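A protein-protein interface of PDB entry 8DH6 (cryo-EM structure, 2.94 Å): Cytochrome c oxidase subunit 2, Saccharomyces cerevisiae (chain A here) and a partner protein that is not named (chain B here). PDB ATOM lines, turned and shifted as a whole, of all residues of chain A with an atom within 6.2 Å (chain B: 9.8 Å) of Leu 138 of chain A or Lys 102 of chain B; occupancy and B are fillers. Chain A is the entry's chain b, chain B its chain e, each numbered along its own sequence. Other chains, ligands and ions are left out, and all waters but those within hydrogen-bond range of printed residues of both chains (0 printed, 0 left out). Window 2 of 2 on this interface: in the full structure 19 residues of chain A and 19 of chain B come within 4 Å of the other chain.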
ATOM      1  N   ILE A 133       9.630  24.364  -2.879  1.00  0.00           N
ATOM      2  CA  ILE A 133      10.459  24.972  -1.834  1.00  0.00           C
ATOM      3  C   ILE A 133      11.822  24.289  -1.818  1.00  0.00           C
ATOM      4  O   ILE A 133      11.890  23.051  -1.719  1.00  0.00           O
ATOM      5  CB  ILE A 133       9.769  24.861  -0.476  1.00  0.00           C
ATOM      6  CG1 ILE A 133       8.498  25.708  -0.470  1.00  0.00           C
ATOM      7  CG2 ILE A 133      10.701  25.312   0.630  1.00  0.00           C
ATOM      8  CD1 ILE A 133       7.772  25.702   0.841  1.00  0.00           C
ATOM      9  N   PRO A 134      12.920  25.032  -1.921  1.00  0.00           N
ATOM     10  CA  PRO A 134      14.243  24.402  -1.935  1.00  0.00           C
ATOM     11  C   PRO A 134      14.555  23.742  -0.601  1.00  0.00           C
ATOM     12  O   PRO A 134      14.032  24.109   0.453  1.00  0.00           O
ATOM     13  CB  PRO A 134      15.195  25.568  -2.220  1.00  0.00           C
ATOM     14  CG  PRO A 134      14.325  26.663  -2.756  1.00  0.00           C
ATOM     15  CD  PRO A 134      13.002  26.489  -2.092  1.00  0.00           C
ATOM     16  N   ASP A 135      15.427  22.733  -0.667  1.00  0.00           N
ATOM     17  CA  ASP A 135      15.794  21.994   0.536  1.00  0.00           C
ATOM     18  C   ASP A 135      16.491  22.889   1.553  1.00  0.00           C
ATOM     19  O   ASP A 135      16.334  22.688   2.763  1.00  0.00           O
ATOM     20  CB  ASP A 135      16.684  20.807   0.173  1.00  0.00           C
ATOM     21  CG  ASP A 135      16.972  19.911   1.359  1.00  0.00           C
ATOM     22  OD1 ASP A 135      16.097  19.791   2.242  1.00  0.00           O
ATOM     23  OD2 ASP A 135      18.075  19.327   1.410  1.00  0.00           O
ATOM     24  N   GLU A 136      17.261  23.874   1.089  1.00  0.00           N
ATOM     25  CA  GLU A 136      17.886  24.826   1.998  1.00  0.00           C
ATOM     26  C   GLU A 136      16.886  25.804   2.597  1.00  0.00           C
ATOM     27  O   GLU A 136      17.171  26.396   3.643  1.00  0.00           O
ATOM     28  CB  GLU A 136      18.986  25.604   1.276  1.00  0.00           C
ATOM     29  CG  GLU A 136      20.166  24.756   0.827  1.00  0.00           C
ATOM     30  CD  GLU A 136      19.947  24.124  -0.534  1.00  0.00           C
ATOM     31  OE1 GLU A 136      18.903  24.404  -1.162  1.00  0.00           O
ATOM     32  OE2 GLU A 136      20.818  23.347  -0.978  1.00  0.00           O
ATOM     33  N   LEU A 137      15.730  25.987   1.961  1.00  0.00           N
ATOM     34  CA  LEU A 137      14.712  26.921   2.424  1.00  0.00           C
ATOM     35  C   LEU A 137      13.548  26.223   3.115  1.00  0.00           C
ATOM     36  O   LEU A 137      12.493  26.838   3.303  1.00  0.00           O
ATOM     37  CB  LEU A 137      14.193  27.768   1.258  1.00  0.00           C
ATOM     38  CG  LEU A 137      14.993  29.007   0.837  1.00  0.00           C
ATOM     39  CD1 LEU A 137      15.011  30.024   1.965  1.00  0.00           C
ATOM     40  CD2 LEU A 137      16.408  28.667   0.383  1.00  0.00           C
ATOM     41  N   LEU A 138      13.706  24.955   3.480  1.00  0.00           N
ATOM     42  CA  LEU A 138      12.642  24.236   4.164  1.00  0.00           C
ATOM     43  C   LEU A 138      12.699  24.498   5.662  1.00  0.00           C
ATOM     44  O   LEU A 138      13.756  24.369   6.287  1.00  0.00           O
ATOM     45  CB  LEU A 138      12.755  22.737   3.896  1.00  0.00           C
ATOM     46  CG  LEU A 138      12.185  22.204   2.584  1.00  0.00           C
ATOM     47  CD1 LEU A 138      12.649  20.784   2.360  1.00  0.00           C
ATOM     48  CD2 LEU A 138      10.676  22.265   2.604  1.00  0.00           C
ATOM     49  N   GLU A 139      11.564  24.868   6.238  1.00  0.00           N
ATOM     50  CA  GLU A 139      11.445  24.939   7.684  1.00  0.00           C
ATOM     51  C   GLU A 139      11.029  23.574   8.225  1.00  0.00           C
ATOM     52  O   GLU A 139      10.366  22.786   7.548  1.00  0.00           O
ATOM     53  CB  GLU A 139      10.452  26.027   8.092  1.00  0.00           C
ATOM     54  CG  GLU A 139       9.022  25.760   7.670  1.00  0.00           C
ATOM     55  CD  GLU A 139       8.084  26.891   8.037  1.00  0.00           C
ATOM     56  OE1 GLU A 139       8.557  27.899   8.603  1.00  0.00           O
ATOM     57  OE2 GLU A 139       6.871  26.773   7.760  1.00  0.00           O
ATOM     58  N   GLU A 140      11.436  23.296   9.461  1.00  0.00           N
ATOM     59  CA  GLU A 140      11.274  21.963  10.028  1.00  0.00           C
ATOM     60  C   GLU A 140       9.797  21.606  10.123  1.00  0.00           C
ATOM     61  O   GLU A 140       9.043  22.239  10.869  1.00  0.00           O
ATOM     62  CB  GLU A 140      11.936  21.888  11.400  1.00  0.00           C
ATOM     63  CG  GLU A 140      11.888  20.509  12.034  1.00  0.00           C
ATOM     64  CD  GLU A 140      12.599  20.455  13.371  1.00  0.00           C
ATOM     65  OE1 GLU A 140      13.115  21.502  13.815  1.00  0.00           O
ATOM     66  OE2 GLU A 140      12.645  19.364  13.976  1.00  0.00           O
ATOM     67  N   GLN A 142       7.962  20.788   6.999  1.00  0.00           N
ATOM     68  CA  GLN A 142       7.498  20.718   5.622  1.00  0.00           C
ATOM     69  C   GLN A 142       8.063  19.486   4.929  1.00  0.00           C
ATOM     70  O   GLN A 142       9.101  18.953   5.326  1.00  0.00           O
ATOM     71  CB  GLN A 142       7.893  21.983   4.868  1.00  0.00           C
ATOM     72  CG  GLN A 142       7.602  23.253   5.640  1.00  0.00           C
ATOM     73  CD  GLN A 142       7.369  24.445   4.742  1.00  0.00           C
ATOM     74  OE1 GLN A 142       8.104  24.665   3.784  1.00  0.00           O
ATOM     75  NE2 GLN A 142       6.341  25.224   5.047  1.00  0.00           N
ATOM     76  N   LEU A 143       7.367  19.034   3.890  1.00  0.00           N
ATOM     77  CA  LEU A 143       7.733  17.806   3.197  1.00  0.00           C
ATOM     78  C   LEU A 143       8.726  18.111   2.083  1.00  0.00           C
ATOM     79  O   LEU A 143       8.481  18.988   1.248  1.00  0.00           O
ATOM     80  CB  LEU A 143       6.488  17.121   2.640  1.00  0.00           C
ATOM     81  CG  LEU A 143       5.549  16.510   3.680  1.00  0.00           C
ATOM     82  CD1 LEU A 143       4.432  17.476   4.038  1.00  0.00           C
ATOM     83  CD2 LEU A 143       4.983  15.198   3.190  1.00  0.00           C
ATOM     84  N   ARG A 144       9.841  17.387   2.068  1.00  0.00           N
ATOM     85  CA  ARG A 144      10.864  17.594   1.052  1.00  0.00           C
ATOM     86  C   ARG A 144      10.366  17.138  -0.313  1.00  0.00           C
ATOM     87  O   ARG A 144       9.710  16.101  -0.436  1.00  0.00           O
ATOM     88  CB  ARG A 144      12.133  16.829   1.419  1.00  0.00           C
ATOM     89  CG  ARG A 144      13.426  17.526   1.046  1.00  0.00           C
ATOM     90  CD  ARG A 144      14.606  16.616   1.312  1.00  0.00           C
ATOM     91  NE  ARG A 144      14.383  15.299   0.732  1.00  0.00           N
ATOM     92  CZ  ARG A 144      14.820  14.927  -0.463  1.00  0.00           C
ATOM     93  NH1 ARG A 144      15.579  15.723  -1.199  1.00  0.00           N
ATOM     94  NH2 ARG A 144      14.492  13.728  -0.929  1.00  0.00           N
ATOM     95  N   LEU A 145      10.681  17.926  -1.342  1.00  0.00           N
ATOM     96  CA  LEU A 145      10.325  17.631  -2.731  1.00  0.00           C
ATOM     97  C   LEU A 145       8.830  17.429  -2.928  1.00  0.00           C
ATOM     98  O   LEU A 145       8.407  16.863  -3.939  1.00  0.00           O
ATOM     99  CB  LEU A 145      11.087  16.410  -3.257  1.00  0.00           C
ATOM    100  CG  LEU A 145      12.368  16.703  -4.035  1.00  0.00           C
ATOM    101  CD1 LEU A 145      13.445  17.235  -3.120  1.00  0.00           C
ATOM    102  CD2 LEU A 145      12.838  15.451  -4.744  1.00  0.00           C
ATOM    103  N   ASP A 147       6.288  19.874  -0.976  1.00  0.00           N
ATOM    104  CA  ASP A 147       5.555  21.066  -0.569  1.00  0.00           C
ATOM    105  C   ASP A 147       6.079  22.248  -1.376  1.00  0.00           C
ATOM    106  O   ASP A 147       7.290  22.485  -1.426  1.00  0.00           O
ATOM    107  CB  ASP A 147       5.709  21.306   0.931  1.00  0.00           C
ATOM    108  CG  ASP A 147       4.683  22.272   1.474  1.00  0.00           C
ATOM    109  OD1 ASP A 147       3.863  22.781   0.681  1.00  0.00           O
ATOM    110  OD2 ASP A 147       4.691  22.522   2.697  1.00  0.00           O
ATOM    111  N   GLN B  99      25.630  11.991   2.561  1.00  0.00           N
ATOM    112  CA  GLN B  99      24.984  12.048   3.889  1.00  0.00           C
ATOM    113  C   GLN B  99      23.482  11.817   3.757  1.00  0.00           C
ATOM    114  O   GLN B  99      22.985  11.893   2.639  1.00  0.00           O
ATOM    115  CB  GLN B  99      25.261  13.417   4.492  1.00  0.00           C
ATOM    116  CG  GLN B  99      26.431  13.438   5.459  1.00  0.00           C
ATOM    117  CD  GLN B  99      27.506  12.455   5.061  1.00  0.00           C
ATOM    118  OE1 GLN B  99      28.208  12.641   4.069  1.00  0.00           O
ATOM    119  NE2 GLN B  99      27.638  11.391   5.835  1.00  0.00           N
ATOM    120  N   ASP B 100      22.778  11.549   4.849  1.00  0.00           N
ATOM    121  CA  ASP B 100      21.335  11.300   4.651  1.00  0.00           C
ATOM    122  C   ASP B 100      20.579  12.620   4.698  1.00  0.00           C
ATOM    123  O   ASP B 100      21.026  13.513   5.395  1.00  0.00           O
ATOM    124  CB  ASP B 100      20.792  10.285   5.649  1.00  0.00           C
ATOM    125  CG  ASP B 100      21.682   9.063   5.787  1.00  0.00           C
ATOM    126  OD1 ASP B 100      22.383   8.737   4.807  1.00  0.00           O
ATOM    127  OD2 ASP B 100      21.669   8.448   6.871  1.00  0.00           O
ATOM    128  N   ALA B 101      19.461  12.708   4.003  1.00  0.00           N
ATOM    129  CA  ALA B 101      18.663  13.919   3.885  1.00  0.00           C
ATOM    130  C   ALA B 101      18.402  14.527   5.259  1.00  0.00           C
ATOM    131  O   ALA B 101      18.341  13.828   6.274  1.00  0.00           O
ATOM    132  CB  ALA B 101      17.338  13.620   3.186  1.00  0.00           C
ATOM    133  N   LYS B 102      18.253  15.852   5.282  1.00  0.00           N
ATOM    134  CA  LYS B 102      17.991  16.550   6.533  1.00  0.00           C
ATOM    135  C   LYS B 102      16.606  16.253   7.090  1.00  0.00           C
ATOM    136  O   LYS B 102      16.383  16.444   8.289  1.00  0.00           O
ATOM    137  CB  LYS B 102      18.150  18.059   6.344  1.00  0.00           C
ATOM    138  CG  LYS B 102      17.183  18.662   5.336  1.00  0.00           C
ATOM    139  CD  LYS B 102      17.369  20.163   5.211  1.00  0.00           C
ATOM    140  CE  LYS B 102      17.282  20.840   6.566  1.00  0.00           C
ATOM    141  NZ  LYS B 102      17.134  22.311   6.431  1.00  0.00           N
ATOM    142  N   THR B 103      15.677  15.793   6.257  1.00  0.00           N
ATOM    143  CA  THR B 103      14.299  15.569   6.673  1.00  0.00           C
ATOM    144  C   THR B 103      14.068  14.176   7.242  1.00  0.00           C
ATOM    145  O   THR B 103      12.935  13.855   7.614  1.00  0.00           O
ATOM    146  CB  THR B 103      13.346  15.811   5.501  1.00  0.00           C
ATOM    147  OG1 THR B 103      13.498  14.764   4.535  1.00  0.00           O
ATOM    148  CG2 THR B 103      13.642  17.144   4.840  1.00  0.00           C
ATOM    149  N   MET B 104      15.101  13.346   7.316  1.00  0.00           N
ATOM    150  CA  MET B 104      14.977  12.000   7.875  1.00  0.00           C
ATOM    151  C   MET B 104      15.359  11.994   9.354  1.00  0.00           C
ATOM    152  O   MET B 104      16.341  11.383   9.774  1.00  0.00           O
ATOM    153  CB  MET B 104      15.825  11.015   7.078  1.00  0.00           C
ATOM    154  CG  MET B 104      15.429  10.899   5.624  1.00  0.00           C
ATOM    155  SD  MET B 104      13.821  10.110   5.460  1.00  0.00           S
ATOM    156  CE  MET B 104      14.287   8.555   4.716  1.00  0.00           C
ATOM    157  N   ASN B 105      14.554  12.693  10.147  1.00  0.00           N
ATOM    158  CA  ASN B 105      14.710  12.713  11.591  1.00  0.00           C
ATOM    159  C   ASN B 105      13.388  12.338  12.234  1.00  0.00           C
ATOM    160  O   ASN B 105      12.329  12.428  11.609  1.00  0.00           O
ATOM    161  CB  ASN B 105      15.148  14.085  12.115  1.00  0.00           C
ATOM    162  CG  ASN B 105      16.257  14.698  11.300  1.00  0.00           C
ATOM    163  OD1 ASN B 105      16.212  15.881  10.971  1.00  0.00           O
ATOM    164  ND2 ASN B 105      17.264  13.899  10.969  1.00  0.00           N
ATOM    165  N   LYS B 106      13.459  11.902  13.490  1.00  0.00           N
ATOM    166  CA  LYS B 106      12.240  11.676  14.255  1.00  0.00           C
ATOM    167  C   LYS B 106      11.503  12.988  14.502  1.00  0.00           C
ATOM    168  O   LYS B 106      10.285  13.072  14.309  1.00  0.00           O
ATOM    169  CB  LYS B 106      12.586  10.991  15.576  1.00  0.00           C
ATOM    170  CG  LYS B 106      11.402  10.554  16.414  1.00  0.00           C
ATOM    171  CD  LYS B 106      10.689   9.381  15.769  1.00  0.00           C
ATOM    172  CE  LYS B 106       9.517   8.909  16.614  1.00  0.00           C
ATOM    173  NZ  LYS B 106       9.964   8.354  17.922  1.00  0.00           N
ATOM    174  N   GLU B 107      12.236  14.030  14.903  1.00  0.00           N
ATOM    175  CA  GLU B 107      11.616  15.306  15.249  1.00  0.00           C
ATOM    176  C   GLU B 107      10.999  15.991  14.036  1.00  0.00           C
ATOM    177  O   GLU B 107       9.879  16.507  14.123  1.00  0.00           O
ATOM    178  CB  GLU B 107      12.646  16.226  15.904  1.00  0.00           C
ATOM    179  CG  GLU B 107      13.428  15.578  17.036  1.00  0.00           C
ATOM    180  CD  GLU B 107      14.650  14.813  16.554  1.00  0.00           C
ATOM    181  OE1 GLU B 107      15.490  14.439  17.398  1.00  0.00           O
ATOM    182  OE2 GLU B 107      14.769  14.584  15.334  1.00  0.00           O
ATOM    183  N   TRP B 108      11.709  16.010  12.907  1.00  0.00           N
ATOM    184  CA  TRP B 108      11.177  16.610  11.688  1.00  0.00           C
ATOM    185  C   TRP B 108       9.896  15.918  11.247  1.00  0.00           C
ATOM    186  O   TRP B 108       8.912  16.578  10.885  1.00  0.00           O
ATOM    187  CB  TRP B 108      12.228  16.534  10.580  1.00  0.00           C
ATOM    188  CG  TRP B 108      11.891  17.277   9.325  1.00  0.00           C
ATOM    189  CD1 TRP B 108      10.904  16.977   8.434  1.00  0.00           C
ATOM    190  CD2 TRP B 108      12.571  18.421   8.796  1.00  0.00           C
ATOM    191  NE1 TRP B 108      10.913  17.875   7.396  1.00  0.00           N
ATOM    192  CE2 TRP B 108      11.929  18.770   7.594  1.00  0.00           C
ATOM    193  CE3 TRP B 108      13.655  19.188   9.229  1.00  0.00           C
ATOM    194  CZ2 TRP B 108      12.334  19.852   6.820  1.00  0.00           C
ATOM    195  CZ3 TRP B 108      14.055  20.261   8.460  1.00  0.00           C
ATOM    196  CH2 TRP B 108      13.396  20.584   7.269  1.00  0.00           C
ATOM    197  N   GLN B 109       9.887  14.591  11.284  1.00  0.00           N
ATOM    198  CA  GLN B 109       8.745  13.843  10.791  1.00  0.00           C
ATOM    199  C   GLN B 109       7.567  13.851  11.756  1.00  0.00           C
ATOM    200  O   GLN B 109       6.423  13.758  11.304  1.00  0.00           O
ATOM    201  CB  GLN B 109       9.182  12.420  10.457  1.00  0.00           C
ATOM    202  CG  GLN B 109      10.189  12.383   9.322  1.00  0.00           C
ATOM    203  CD  GLN B 109      10.604  10.983   8.949  1.00  0.00           C
ATOM    204  OE1 GLN B 109       9.961  10.333   8.128  1.00  0.00           O
ATOM    205  NE2 GLN B 109      11.681  10.504   9.554  1.00  0.00           N
ATOM    206  N   SER B 112       6.004  17.036  10.715  1.00  0.00           N
ATOM    207  CA  SER B 112       5.289  16.810   9.462  1.00  0.00           C
ATOM    208  C   SER B 112       3.972  16.081   9.704  1.00  0.00           C
ATOM    209  O   SER B 112       2.948  16.410   9.090  1.00  0.00           O
ATOM    210  CB  SER B 112       6.168  16.027   8.490  1.00  0.00           C
ATOM    211  OG  SER B 112       5.499  15.822   7.260  1.00  0.00           O
ATOM    212  N   SER B 132      11.826   6.356  10.759  1.00  0.00           N
ATOM    213  CA  SER B 132      13.212   6.677  11.062  1.00  0.00           C
ATOM    214  C   SER B 132      13.337   7.063  12.527  1.00  0.00           C
ATOM    215  O   SER B 132      12.343   7.282  13.224  1.00  0.00           O
ATOM    216  CB  SER B 132      13.731   7.802  10.163  1.00  0.00           C
ATOM    217  OG  SER B 132      15.064   8.141  10.492  1.00  0.00           O
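The side-chain amide nitrogen (NE2) of Gln 142 of chain A lies within hydrogen-bond range of the side-chain carboxylate (OE2) of Glu 139 of chain A (3.2 Å). The backbone carbonyl oxygen of Lys 102 of chain B sits close to the side-chain amide oxygen of Asn 105 of chain B (2.7 Å).
NE1 of Trp 108 of chain B lies within hydrogen-bond range of O of Gln 142 of chain A, 3.0 Å away.
Ile 133 of chain A touches none of the printed residues of chain B. Pro 134 of chain A touches none of the printed residues of chain B. Of chain B, only Lys 102 and Trp 108 come within 4 Å of Leu 138 of chain A. Printed residues of chain B within 4 Å of Glu 140 of chain A: Glu 107 (3.7 Å) and Trp 108 (3.6 Å). Of the printed residues of chain B, Leu 143 of chain A touches Ser 112 (3.6 Å). Of chain A, only Asp 135 (3.3 Å) and Leu 138 (3.96 Å) come within 4 Å of Lys 102 of chain B. Printed residues of chain A within 4 Å of Thr 103 of chain B: Arg 144. Of the printed residues of chain A, Glu 107 of chain B touches Glu 140 (3.7 Å). The nearest residue of chain B that does not touch Leu 138 of chain A is Thr 103 of chain B (4.5 Å). The nearest residue of chain A that does not touch Lys 102 of chain B is Glu 136 of chain A (4.9 Å). The nearest printed residue of chain A that does not touch Trp 108 of chain B is Leu 143 of chain A (5.1 Å).
Among the printed residues, pairs that only touch across the chains: Asp 135 of chain A with Lys 102 of chain B, Glu 140 of chain A with Trp 108 of chain B, Glu 139 of chain A with Trp 108 of chain B, Leu 143 of chain A with Ser 112 of chain B, Glu 140 of chain A with Glu 107 of chain B, Arg 144 of chain A with Thr 103 of chain B, Leu 138 of chain A with Trp 108 of chain B and Leu 138 of chain A with Lys 102 of chain B.
Hydrophobic or aromatic side chains of chain B within 4 Å of the printed part of chain A: Trp 108. Hydrophobic or aromatic side chains of chain A that line the printed part of chain B: Leu 143. Among the printed residues, 9 pairs touch across the chains. Among the printed residues, no Asp or Glu carboxylate lies within 4 Å of a Lys or Arg side-chain nitrogen of the other chain.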
